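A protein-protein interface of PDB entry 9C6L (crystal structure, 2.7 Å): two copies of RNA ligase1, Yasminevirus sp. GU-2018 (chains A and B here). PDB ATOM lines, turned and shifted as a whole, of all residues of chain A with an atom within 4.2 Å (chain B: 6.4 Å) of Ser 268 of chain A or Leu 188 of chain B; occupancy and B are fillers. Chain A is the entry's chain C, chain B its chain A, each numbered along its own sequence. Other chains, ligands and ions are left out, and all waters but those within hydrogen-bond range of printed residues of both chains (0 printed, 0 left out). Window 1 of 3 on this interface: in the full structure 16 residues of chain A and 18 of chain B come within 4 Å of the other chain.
Hydrophobic or aromatic side chains of chain A within 4 Å of the printed part of chain B: Pro 238.
Of the 19 printed residues of chain B, 5 touch a printed residue of chain A.
Hydrophobic or aromatic side chains of chain B within 4 Å of the printed part of chain A: Pro 179.
Among the printed residues, no Asp or Glu carboxylate lies within 4 Å of a Lys or Arg side-chain nitrogen of the other chain.
OH of Tyr 161 of chain B is in hydrogen-bond range of N of Lys 189 of chain B, 3.3 Å away.
O of Leu 188 of chain B sits at hydrogen-bond distance from ND2 of Asn 184 of chain B.
NZ of Lys 189 of chain B lies within salt-bridge range of OD2 of Asp 273 of chain B, at 3.3 Å.
The guanidinium group of Arg 257 of chain A lies within hydrogen-bond range of the backbone carbonyl oxygen of Pro 238 of chain A (3.0 Å).
The guanidinium group of Arg 257 of chain A lies within hydrogen-bond range of the backbone carbonyl oxygen of Glu 263 of chain A (2.6 Å).
The guanidinium group (NH1) of Arg 257 of chain A is in hydrogen-bond range of the backbone carbonyl oxygen (O) of Ser 268 of chain A.
Of the printed residues of chain B, Pro 238 of chain A touches Lys 189 (3.8 Å).
Printed residues of chain B within 4 Å of Glu 263 of chain A: Pro 179 and Lys 189.
Ser 268 of chain A touches just these residues of chain B: Gly 187, Leu 188 and Lys 189.
Of the printed residues of chain A, Asn 184 of chain B touches Lys 267 (3.6 Å).
Of the printed residues of chain A, Gly 187 of chain B touches Lys 267 (3.4 Å) and Ser 268 (3.9 Å).
The nearest residue of chain B that does not touch Ser 268 of chain A is Asn 184 of chain B (4.6 Å).
The nearest printed residue of chain A that does not touch Leu 188 of chain B is Glu 263 of chain A (4.6 Å).
CB of Pro 238 of chain A touches NZ of Lys 189 of chain B (3.8 Å).
NH1 of Arg 257 of chain A touches CG of Lys 189 of chain B (3.6 Å).
Glu 263 of chain A touches Pro 179 of chain B.
Asn 184 of chain B touches Lys 267 of chain A.
Lys 267 of chain A touches Gly 187 of chain B.
Ser 268 of chain A touches Gly 187 of chain B (CA to O, 3.9 Å).
CB of Ser 268 of chain A touches O of Leu 188 of chain B (3.5 Å).
Ser 268 of chain A touches Lys 189 of chain B (O to CG, 3.5 Å).
N of Glu 263 of chain A lies within hydrogen-bond range of O of Lys 189 of chain B (2.9 Å).
No position is printed for both chains.
Of the 9 pairs that touch across the chains among the printed residues, none has its exchanged pair printed and touching as well.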
ATOM      1  N   PRO A 238      20.117 -24.459   5.228  1.00  0.00           N
ATOM      2  CA  PRO A 238      19.499 -23.128   5.087  1.00  0.00           C
ATOM      3  C   PRO A 238      20.483 -22.008   4.778  1.00  0.00           C
ATOM      4  O   PRO A 238      20.047 -20.932   4.350  1.00  0.00           O
ATOM      5  CB  PRO A 238      18.808 -22.909   6.444  1.00  0.00           C
ATOM      6  CG  PRO A 238      19.325 -23.977   7.350  1.00  0.00           C
ATOM      7  CD  PRO A 238      19.710 -25.122   6.478  1.00  0.00           C
ATOM      8  N   ARG A 257      19.463 -25.491  -5.261  1.00  0.00           N
ATOM      9  CA  ARG A 257      18.177 -25.574  -4.577  1.00  0.00           C
ATOM     10  C   ARG A 257      17.017 -25.728  -5.553  1.00  0.00           C
ATOM     11  O   ARG A 257      15.948 -26.201  -5.157  1.00  0.00           O
ATOM     12  CB  ARG A 257      17.946 -24.333  -3.716  1.00  0.00           C
ATOM     13  CG  ARG A 257      18.508 -24.413  -2.304  1.00  0.00           C
ATOM     14  CD  ARG A 257      17.811 -23.399  -1.408  1.00  0.00           C
ATOM     15  NE  ARG A 257      18.529 -23.134  -0.167  1.00  0.00           N
ATOM     16  CZ  ARG A 257      18.151 -22.236   0.734  1.00  0.00           C
ATOM     17  NH1 ARG A 257      17.056 -21.511   0.571  1.00  0.00           N
ATOM     18  NH2 ARG A 257      18.891 -22.058   1.825  1.00  0.00           N
ATOM     19  N   GLU A 263      13.489 -22.743  -2.720  1.00  0.00           N
ATOM     20  CA  GLU A 263      13.668 -21.332  -3.022  1.00  0.00           C
ATOM     21  C   GLU A 263      15.046 -20.871  -2.568  1.00  0.00           C
ATOM     22  O   GLU A 263      15.519 -21.257  -1.495  1.00  0.00           O
ATOM     23  CB  GLU A 263      12.581 -20.510  -2.324  1.00  0.00           C
ATOM     24  CG  GLU A 263      12.651 -19.004  -2.550  1.00  0.00           C
ATOM     25  CD  GLU A 263      11.858 -18.546  -3.757  1.00  0.00           C
ATOM     26  OE1 GLU A 263      11.313 -19.408  -4.482  1.00  0.00           O
ATOM     27  OE2 GLU A 263      11.777 -17.319  -3.978  1.00  0.00           O
ATOM     28  N   TRP A 264      15.690 -20.044  -3.390  1.00  0.00           N
ATOM     29  CA  TRP A 264      16.966 -19.427  -3.043  1.00  0.00           C
ATOM     30  C   TRP A 264      16.829 -17.916  -3.141  1.00  0.00           C
ATOM     31  O   TRP A 264      16.475 -17.386  -4.201  1.00  0.00           O
ATOM     32  CB  TRP A 264      18.097 -19.919  -3.947  1.00  0.00           C
ATOM     33  CG  TRP A 264      19.418 -19.315  -3.577  1.00  0.00           C
ATOM     34  CD1 TRP A 264      20.238 -18.579  -4.379  1.00  0.00           C
ATOM     35  CD2 TRP A 264      20.060 -19.380  -2.297  1.00  0.00           C
ATOM     36  NE1 TRP A 264      21.357 -18.191  -3.682  1.00  0.00           N
ATOM     37  CE2 TRP A 264      21.270 -18.668  -2.401  1.00  0.00           C
ATOM     38  CE3 TRP A 264      19.729 -19.975  -1.077  1.00  0.00           C
ATOM     39  CZ2 TRP A 264      22.151 -18.534  -1.331  1.00  0.00           C
ATOM     40  CZ3 TRP A 264      20.605 -19.842  -0.017  1.00  0.00           C
ATOM     41  CH2 TRP A 264      21.801 -19.126  -0.150  1.00  0.00           C
ATOM     42  N   SER A 265      17.124 -17.227  -2.043  1.00  0.00           N
ATOM     43  CA  SER A 265      16.949 -15.786  -1.930  1.00  0.00           C
ATOM     44  C   SER A 265      17.442 -15.369  -0.554  1.00  0.00           C
ATOM     45  O   SER A 265      17.565 -16.198   0.353  1.00  0.00           O
ATOM     46  CB  SER A 265      15.487 -15.372  -2.116  1.00  0.00           C
ATOM     47  OG  SER A 265      14.682 -15.894  -1.072  1.00  0.00           O
ATOM     48  N   ALA A 266      17.723 -14.073  -0.406  1.00  0.00           N
ATOM     49  CA  ALA A 266      18.153 -13.570   0.894  1.00  0.00           C
ATOM     50  C   ALA A 266      17.109 -13.848   1.968  1.00  0.00           C
ATOM     51  O   ALA A 266      17.456 -14.021   3.141  1.00  0.00           O
ATOM     52  CB  ALA A 266      18.449 -12.073   0.809  1.00  0.00           C
ATOM     53  N   LYS A 267      15.830 -13.900   1.586  1.00  0.00           N
ATOM     54  CA  LYS A 267      14.779 -14.207   2.552  1.00  0.00           C
ATOM     55  C   LYS A 267      14.845 -15.664   2.994  1.00  0.00           C
ATOM     56  O   LYS A 267      14.798 -15.962   4.193  1.00  0.00           O
ATOM     57  CB  LYS A 267      13.407 -13.895   1.953  1.00  0.00           C
ATOM     58  CG  LYS A 267      12.853 -12.533   2.327  1.00  0.00           C
ATOM     59  CD  LYS A 267      11.464 -12.335   1.742  1.00  0.00           C
ATOM     60  CE  LYS A 267      11.361 -11.032   0.969  1.00  0.00           C
ATOM     61  NZ  LYS A 267      10.200 -11.038   0.035  1.00  0.00           N
ATOM     62  N   SER A 268      14.947 -16.586   2.040  1.00  0.00           N
ATOM     63  CA  SER A 268      14.996 -18.009   2.348  1.00  0.00           C
ATOM     64  C   SER A 268      16.392 -18.485   2.734  1.00  0.00           C
ATOM     65  O   SER A 268      16.596 -19.694   2.892  1.00  0.00           O
ATOM     66  CB  SER A 268      14.486 -18.824   1.155  1.00  0.00           C
ATOM     67  OG  SER A 268      15.389 -18.758   0.065  1.00  0.00           O
ATOM     68  N   ALA A 269      17.347 -17.572   2.897  1.00  0.00           N
ATOM     69  CA  ALA A 269      18.728 -17.918   3.198  1.00  0.00           C
ATOM     70  C   ALA A 269      19.144 -17.255   4.502  1.00  0.00           C
ATOM     71  O   ALA A 269      18.896 -16.063   4.703  1.00  0.00           O
ATOM     72  CB  ALA A 269      19.662 -17.477   2.069  1.00  0.00           C
ATOM     73  N   THR B  75       0.274 -17.394  11.790  1.00  0.00           N
ATOM     74  CA  THR B  75       1.220 -17.335  10.687  1.00  0.00           C
ATOM     75  C   THR B  75       0.559 -16.635   9.505  1.00  0.00           C
ATOM     76  O   THR B  75      -0.667 -16.537   9.423  1.00  0.00           O
ATOM     77  CB  THR B  75       1.705 -18.741  10.300  1.00  0.00           C
ATOM     78  OG1 THR B  75       2.822 -18.640   9.409  1.00  0.00           O
ATOM     79  CG2 THR B  75       0.598 -19.537   9.631  1.00  0.00           C
ATOM     80  N   ASP B  76       1.381 -16.130   8.591  1.00  0.00           N
ATOM     81  CA  ASP B  76       0.915 -15.268   7.509  1.00  0.00           C
ATOM     82  C   ASP B  76       0.963 -16.042   6.200  1.00  0.00           C
ATOM     83  O   ASP B  76       2.044 -16.357   5.692  1.00  0.00           O
ATOM     84  CB  ASP B  76       1.755 -13.997   7.418  1.00  0.00           C
ATOM     85  CG  ASP B  76       1.144 -12.963   6.491  1.00  0.00           C
ATOM     86  OD1 ASP B  76       0.023 -13.201   5.992  1.00  0.00           O
ATOM     87  OD2 ASP B  76       1.783 -11.913   6.265  1.00  0.00           O
ATOM     88  N   ILE B 150       5.065 -27.903   7.215  1.00  0.00           N
ATOM     89  CA  ILE B 150       5.955 -27.526   8.306  1.00  0.00           C
ATOM     90  C   ILE B 150       5.214 -27.801   9.607  1.00  0.00           C
ATOM     91  O   ILE B 150       4.121 -27.267   9.834  1.00  0.00           O
ATOM     92  CB  ILE B 150       6.400 -26.058   8.201  1.00  0.00           C
ATOM     93  CG1 ILE B 150       7.389 -25.718   9.317  1.00  0.00           C
ATOM     94  CG2 ILE B 150       5.206 -25.114   8.248  1.00  0.00           C
ATOM     95  CD1 ILE B 150       8.156 -24.436   9.076  1.00  0.00           C
ATOM     96  N   TYR B 161      10.482 -29.160   8.220  1.00  0.00           N
ATOM     97  CA  TYR B 161       9.755 -29.459   6.995  1.00  0.00           C
ATOM     98  C   TYR B 161       9.635 -30.971   6.859  1.00  0.00           C
ATOM     99  O   TYR B 161      10.618 -31.697   7.045  1.00  0.00           O
ATOM    100  CB  TYR B 161      10.472 -28.885   5.774  1.00  0.00           C
ATOM    101  CG  TYR B 161      10.713 -27.390   5.806  1.00  0.00           C
ATOM    102  CD1 TYR B 161      11.802 -26.854   6.483  1.00  0.00           C
ATOM    103  CD2 TYR B 161       9.865 -26.517   5.134  1.00  0.00           C
ATOM    104  CE1 TYR B 161      12.031 -25.490   6.503  1.00  0.00           C
ATOM    105  CE2 TYR B 161      10.086 -25.153   5.149  1.00  0.00           C
ATOM    106  CZ  TYR B 161      11.170 -24.644   5.833  1.00  0.00           C
ATOM    107  OH  TYR B 161      11.391 -23.285   5.848  1.00  0.00           O
ATOM    108  N   MET B 177       1.819 -21.280   2.954  1.00  0.00           N
ATOM    109  CA  MET B 177       2.841 -20.252   3.075  1.00  0.00           C
ATOM    110  C   MET B 177       3.960 -20.534   2.083  1.00  0.00           C
ATOM    111  O   MET B 177       4.038 -21.615   1.492  1.00  0.00           O
ATOM    112  CB  MET B 177       3.399 -20.199   4.504  1.00  0.00           C
ATOM    113  CG  MET B 177       2.330 -20.090   5.585  1.00  0.00           C
ATOM    114  SD  MET B 177       2.965 -20.426   7.239  1.00  0.00           S
ATOM    115  CE  MET B 177       3.342 -22.172   7.120  1.00  0.00           C
ATOM    116  N   GLY B 178       4.832 -19.544   1.898  1.00  0.00           N
ATOM    117  CA  GLY B 178       5.999 -19.710   1.065  1.00  0.00           C
ATOM    118  C   GLY B 178       6.339 -18.494   0.225  1.00  0.00           C
ATOM    119  O   GLY B 178       5.762 -17.412   0.379  1.00  0.00           O
ATOM    120  N   PRO B 179       7.304 -18.662  -0.693  1.00  0.00           N
ATOM    121  CA  PRO B 179       7.761 -17.545  -1.535  1.00  0.00           C
ATOM    122  C   PRO B 179       6.667 -16.653  -2.106  1.00  0.00           C
ATOM    123  O   PRO B 179       6.721 -15.429  -1.947  1.00  0.00           O
ATOM    124  CB  PRO B 179       8.521 -18.269  -2.653  1.00  0.00           C
ATOM    125  CG  PRO B 179       9.111 -19.460  -1.964  1.00  0.00           C
ATOM    126  CD  PRO B 179       8.119 -19.874  -0.897  1.00  0.00           C
ATOM    127  N   ASN B 184       6.592 -14.051   1.417  1.00  0.00           N
ATOM    128  CA  ASN B 184       7.343 -14.961   2.275  1.00  0.00           C
ATOM    129  C   ASN B 184       7.897 -14.229   3.501  1.00  0.00           C
ATOM    130  O   ASN B 184       9.110 -14.226   3.732  1.00  0.00           O
ATOM    131  CB  ASN B 184       8.461 -15.649   1.501  1.00  0.00           C
ATOM    132  CG  ASN B 184       9.037 -16.849   2.234  1.00  0.00           C
ATOM    133  OD1 ASN B 184       8.479 -17.322   3.228  1.00  0.00           O
ATOM    134  ND2 ASN B 184      10.160 -17.356   1.733  1.00  0.00           N
ATOM    135  N   PRO B 185       7.030 -13.618   4.316  1.00  0.00           N
ATOM    136  CA  PRO B 185       7.526 -12.920   5.513  1.00  0.00           C
ATOM    137  C   PRO B 185       8.212 -13.839   6.504  1.00  0.00           C
ATOM    138  O   PRO B 185       8.978 -13.354   7.346  1.00  0.00           O
ATOM    139  CB  PRO B 185       6.255 -12.299   6.109  1.00  0.00           C
ATOM    140  CG  PRO B 185       5.137 -13.143   5.592  1.00  0.00           C
ATOM    141  CD  PRO B 185       5.559 -13.589   4.224  1.00  0.00           C
ATOM    142  N   HIS B 186       7.968 -15.147   6.429  1.00  0.00           N
ATOM    143  CA  HIS B 186       8.561 -16.111   7.346  1.00  0.00           C
ATOM    144  C   HIS B 186       9.862 -16.706   6.829  1.00  0.00           C
ATOM    145  O   HIS B 186      10.415 -17.599   7.478  1.00  0.00           O
ATOM    146  CB  HIS B 186       7.570 -17.240   7.630  1.00  0.00           C
ATOM    147  CG  HIS B 186       6.352 -16.795   8.374  1.00  0.00           C
ATOM    148  ND1 HIS B 186       6.402 -16.327   9.669  1.00  0.00           N
ATOM    149  CD2 HIS B 186       5.051 -16.743   8.004  1.00  0.00           C
ATOM    150  CE1 HIS B 186       5.183 -16.008  10.066  1.00  0.00           C
ATOM    151  NE2 HIS B 186       4.347 -16.249   9.073  1.00  0.00           N
ATOM    152  N   GLY B 187      10.362 -16.241   5.689  1.00  0.00           N
ATOM    153  CA  GLY B 187      11.613 -16.764   5.163  1.00  0.00           C
ATOM    154  C   GLY B 187      11.601 -18.263   4.969  1.00  0.00           C
ATOM    155  O   GLY B 187      12.583 -18.939   5.299  1.00  0.00           O
ATOM    156  N   LEU B 188      10.504 -18.801   4.442  1.00  0.00           N
ATOM    157  CA  LEU B 188      10.398 -20.232   4.206  1.00  0.00           C
ATOM    158  C   LEU B 188      11.137 -20.617   2.930  1.00  0.00           C
ATOM    159  O   LEU B 188      11.243 -19.831   1.985  1.00  0.00           O
ATOM    160  CB  LEU B 188       8.930 -20.648   4.113  1.00  0.00           C
ATOM    161  CG  LEU B 188       8.112 -20.406   5.384  1.00  0.00           C
ATOM    162  CD1 LEU B 188       6.628 -20.597   5.121  1.00  0.00           C
ATOM    163  CD2 LEU B 188       8.579 -21.327   6.499  1.00  0.00           C
ATOM    164  N   LYS B 189      11.652 -21.842   2.913  1.00  0.00           N
ATOM    165  CA  LYS B 189      12.448 -22.334   1.797  1.00  0.00           C
ATOM    166  C   LYS B 189      11.617 -23.015   0.716  1.00  0.00           C
ATOM    167  O   LYS B 189      12.191 -23.502  -0.264  1.00  0.00           O
ATOM    168  CB  LYS B 189      13.518 -23.306   2.308  1.00  0.00           C
ATOM    169  CG  LYS B 189      14.671 -22.630   3.031  1.00  0.00           C
ATOM    170  CD  LYS B 189      15.641 -23.646   3.619  1.00  0.00           C
ATOM    171  CE  LYS B 189      15.154 -24.185   4.956  1.00  0.00           C
ATOM    172  NZ  LYS B 189      15.072 -23.119   5.997  1.00  0.00           N
ATOM    173  N   ALA B 190      10.295 -23.064   0.860  1.00  0.00           N
ATOM    174  CA  ALA B 190       9.445 -23.698  -0.140  1.00  0.00           C
ATOM    175  C   ALA B 190       7.991 -23.542   0.280  1.00  0.00           C
ATOM    176  O   ALA B 190       7.687 -23.234   1.436  1.00  0.00           O
ATOM    177  CB  ALA B 190       9.781 -25.182  -0.318  1.00  0.00           C
ATOM    178  N   HIS B 191       7.097 -23.767  -0.680  1.00  0.00           N
ATOM    179  CA  HIS B 191       5.666 -23.696  -0.416  1.00  0.00           C
ATOM    180  C   HIS B 191       5.234 -24.904   0.402  1.00  0.00           C
ATOM    181  O   HIS B 191       5.394 -26.048  -0.034  1.00  0.00           O
ATOM    182  CB  HIS B 191       4.898 -23.625  -1.732  1.00  0.00           C
ATOM    183  CG  HIS B 191       5.127 -22.356  -2.490  1.00  0.00           C
ATOM    184  ND1 HIS B 191       5.537 -22.335  -3.806  1.00  0.00           N
ATOM    185  CD2 HIS B 191       5.005 -21.061  -2.113  1.00  0.00           C
ATOM    186  CE1 HIS B 191       5.659 -21.083  -4.207  1.00  0.00           C
ATOM    187  NE2 HIS B 191       5.343 -20.290  -3.198  1.00  0.00           N
ATOM    188  N   CYS B 192       4.683 -24.651   1.587  1.00  0.00           N
ATOM    189  CA  CYS B 192       4.350 -25.713   2.522  1.00  0.00           C
ATOM    190  C   CYS B 192       3.073 -25.361   3.272  1.00  0.00           C
ATOM    191  O   CYS B 192       2.656 -24.201   3.328  1.00  0.00           O
ATOM    192  CB  CYS B 192       5.494 -25.949   3.515  1.00  0.00           C
ATOM    193  SG  CYS B 192       6.027 -24.450   4.368  1.00  0.00           S
ATOM    194  N   PRO B 271      12.976 -15.736  10.898  1.00  0.00           N
ATOM    195  CA  PRO B 271      12.454 -16.876  10.134  1.00  0.00           C
ATOM    196  C   PRO B 271      11.639 -17.820  11.005  1.00  0.00           C
ATOM    197  O   PRO B 271      12.037 -18.175  12.116  1.00  0.00           O
ATOM    198  CB  PRO B 271      13.720 -17.553   9.599  1.00  0.00           C
ATOM    199  CG  PRO B 271      14.748 -16.483   9.577  1.00  0.00           C
ATOM    200  CD  PRO B 271      14.429 -15.567  10.719  1.00  0.00           C
ATOM    201  N   LEU B 272      10.477 -18.223  10.490  1.00  0.00           N
ATOM    202  CA  LEU B 272       9.623 -19.144  11.230  1.00  0.00           C
ATOM    203  C   LEU B 272      10.327 -20.472  11.478  1.00  0.00           C
ATOM    204  O   LEU B 272      10.154 -21.084  12.537  1.00  0.00           O
ATOM    205  CB  LEU B 272       8.316 -19.364  10.467  1.00  0.00           C
ATOM    206  CG  LEU B 272       7.304 -20.331  11.083  1.00  0.00           C
ATOM    207  CD1 LEU B 272       6.942 -19.912  12.500  1.00  0.00           C
ATOM    208  CD2 LEU B 272       6.060 -20.410  10.210  1.00  0.00           C
ATOM    209  N   ASP B 273      11.134 -20.930  10.516  1.00  0.00           N
ATOM    210  CA  ASP B 273      11.739 -22.253  10.627  1.00  0.00           C
ATOM    211  C   ASP B 273      12.739 -22.352  11.774  1.00  0.00           C
ATOM    212  O   ASP B 273      13.060 -23.467  12.196  1.00  0.00           O
ATOM    213  CB  ASP B 273      12.420 -22.644   9.310  1.00  0.00           C
ATOM    214  CG  ASP B 273      13.427 -21.613   8.837  1.00  0.00           C
ATOM    215  OD1 ASP B 273      14.434 -21.388   9.541  1.00  0.00           O
ATOM    216  OD2 ASP B 273      13.214 -21.036   7.750  1.00  0.00           O
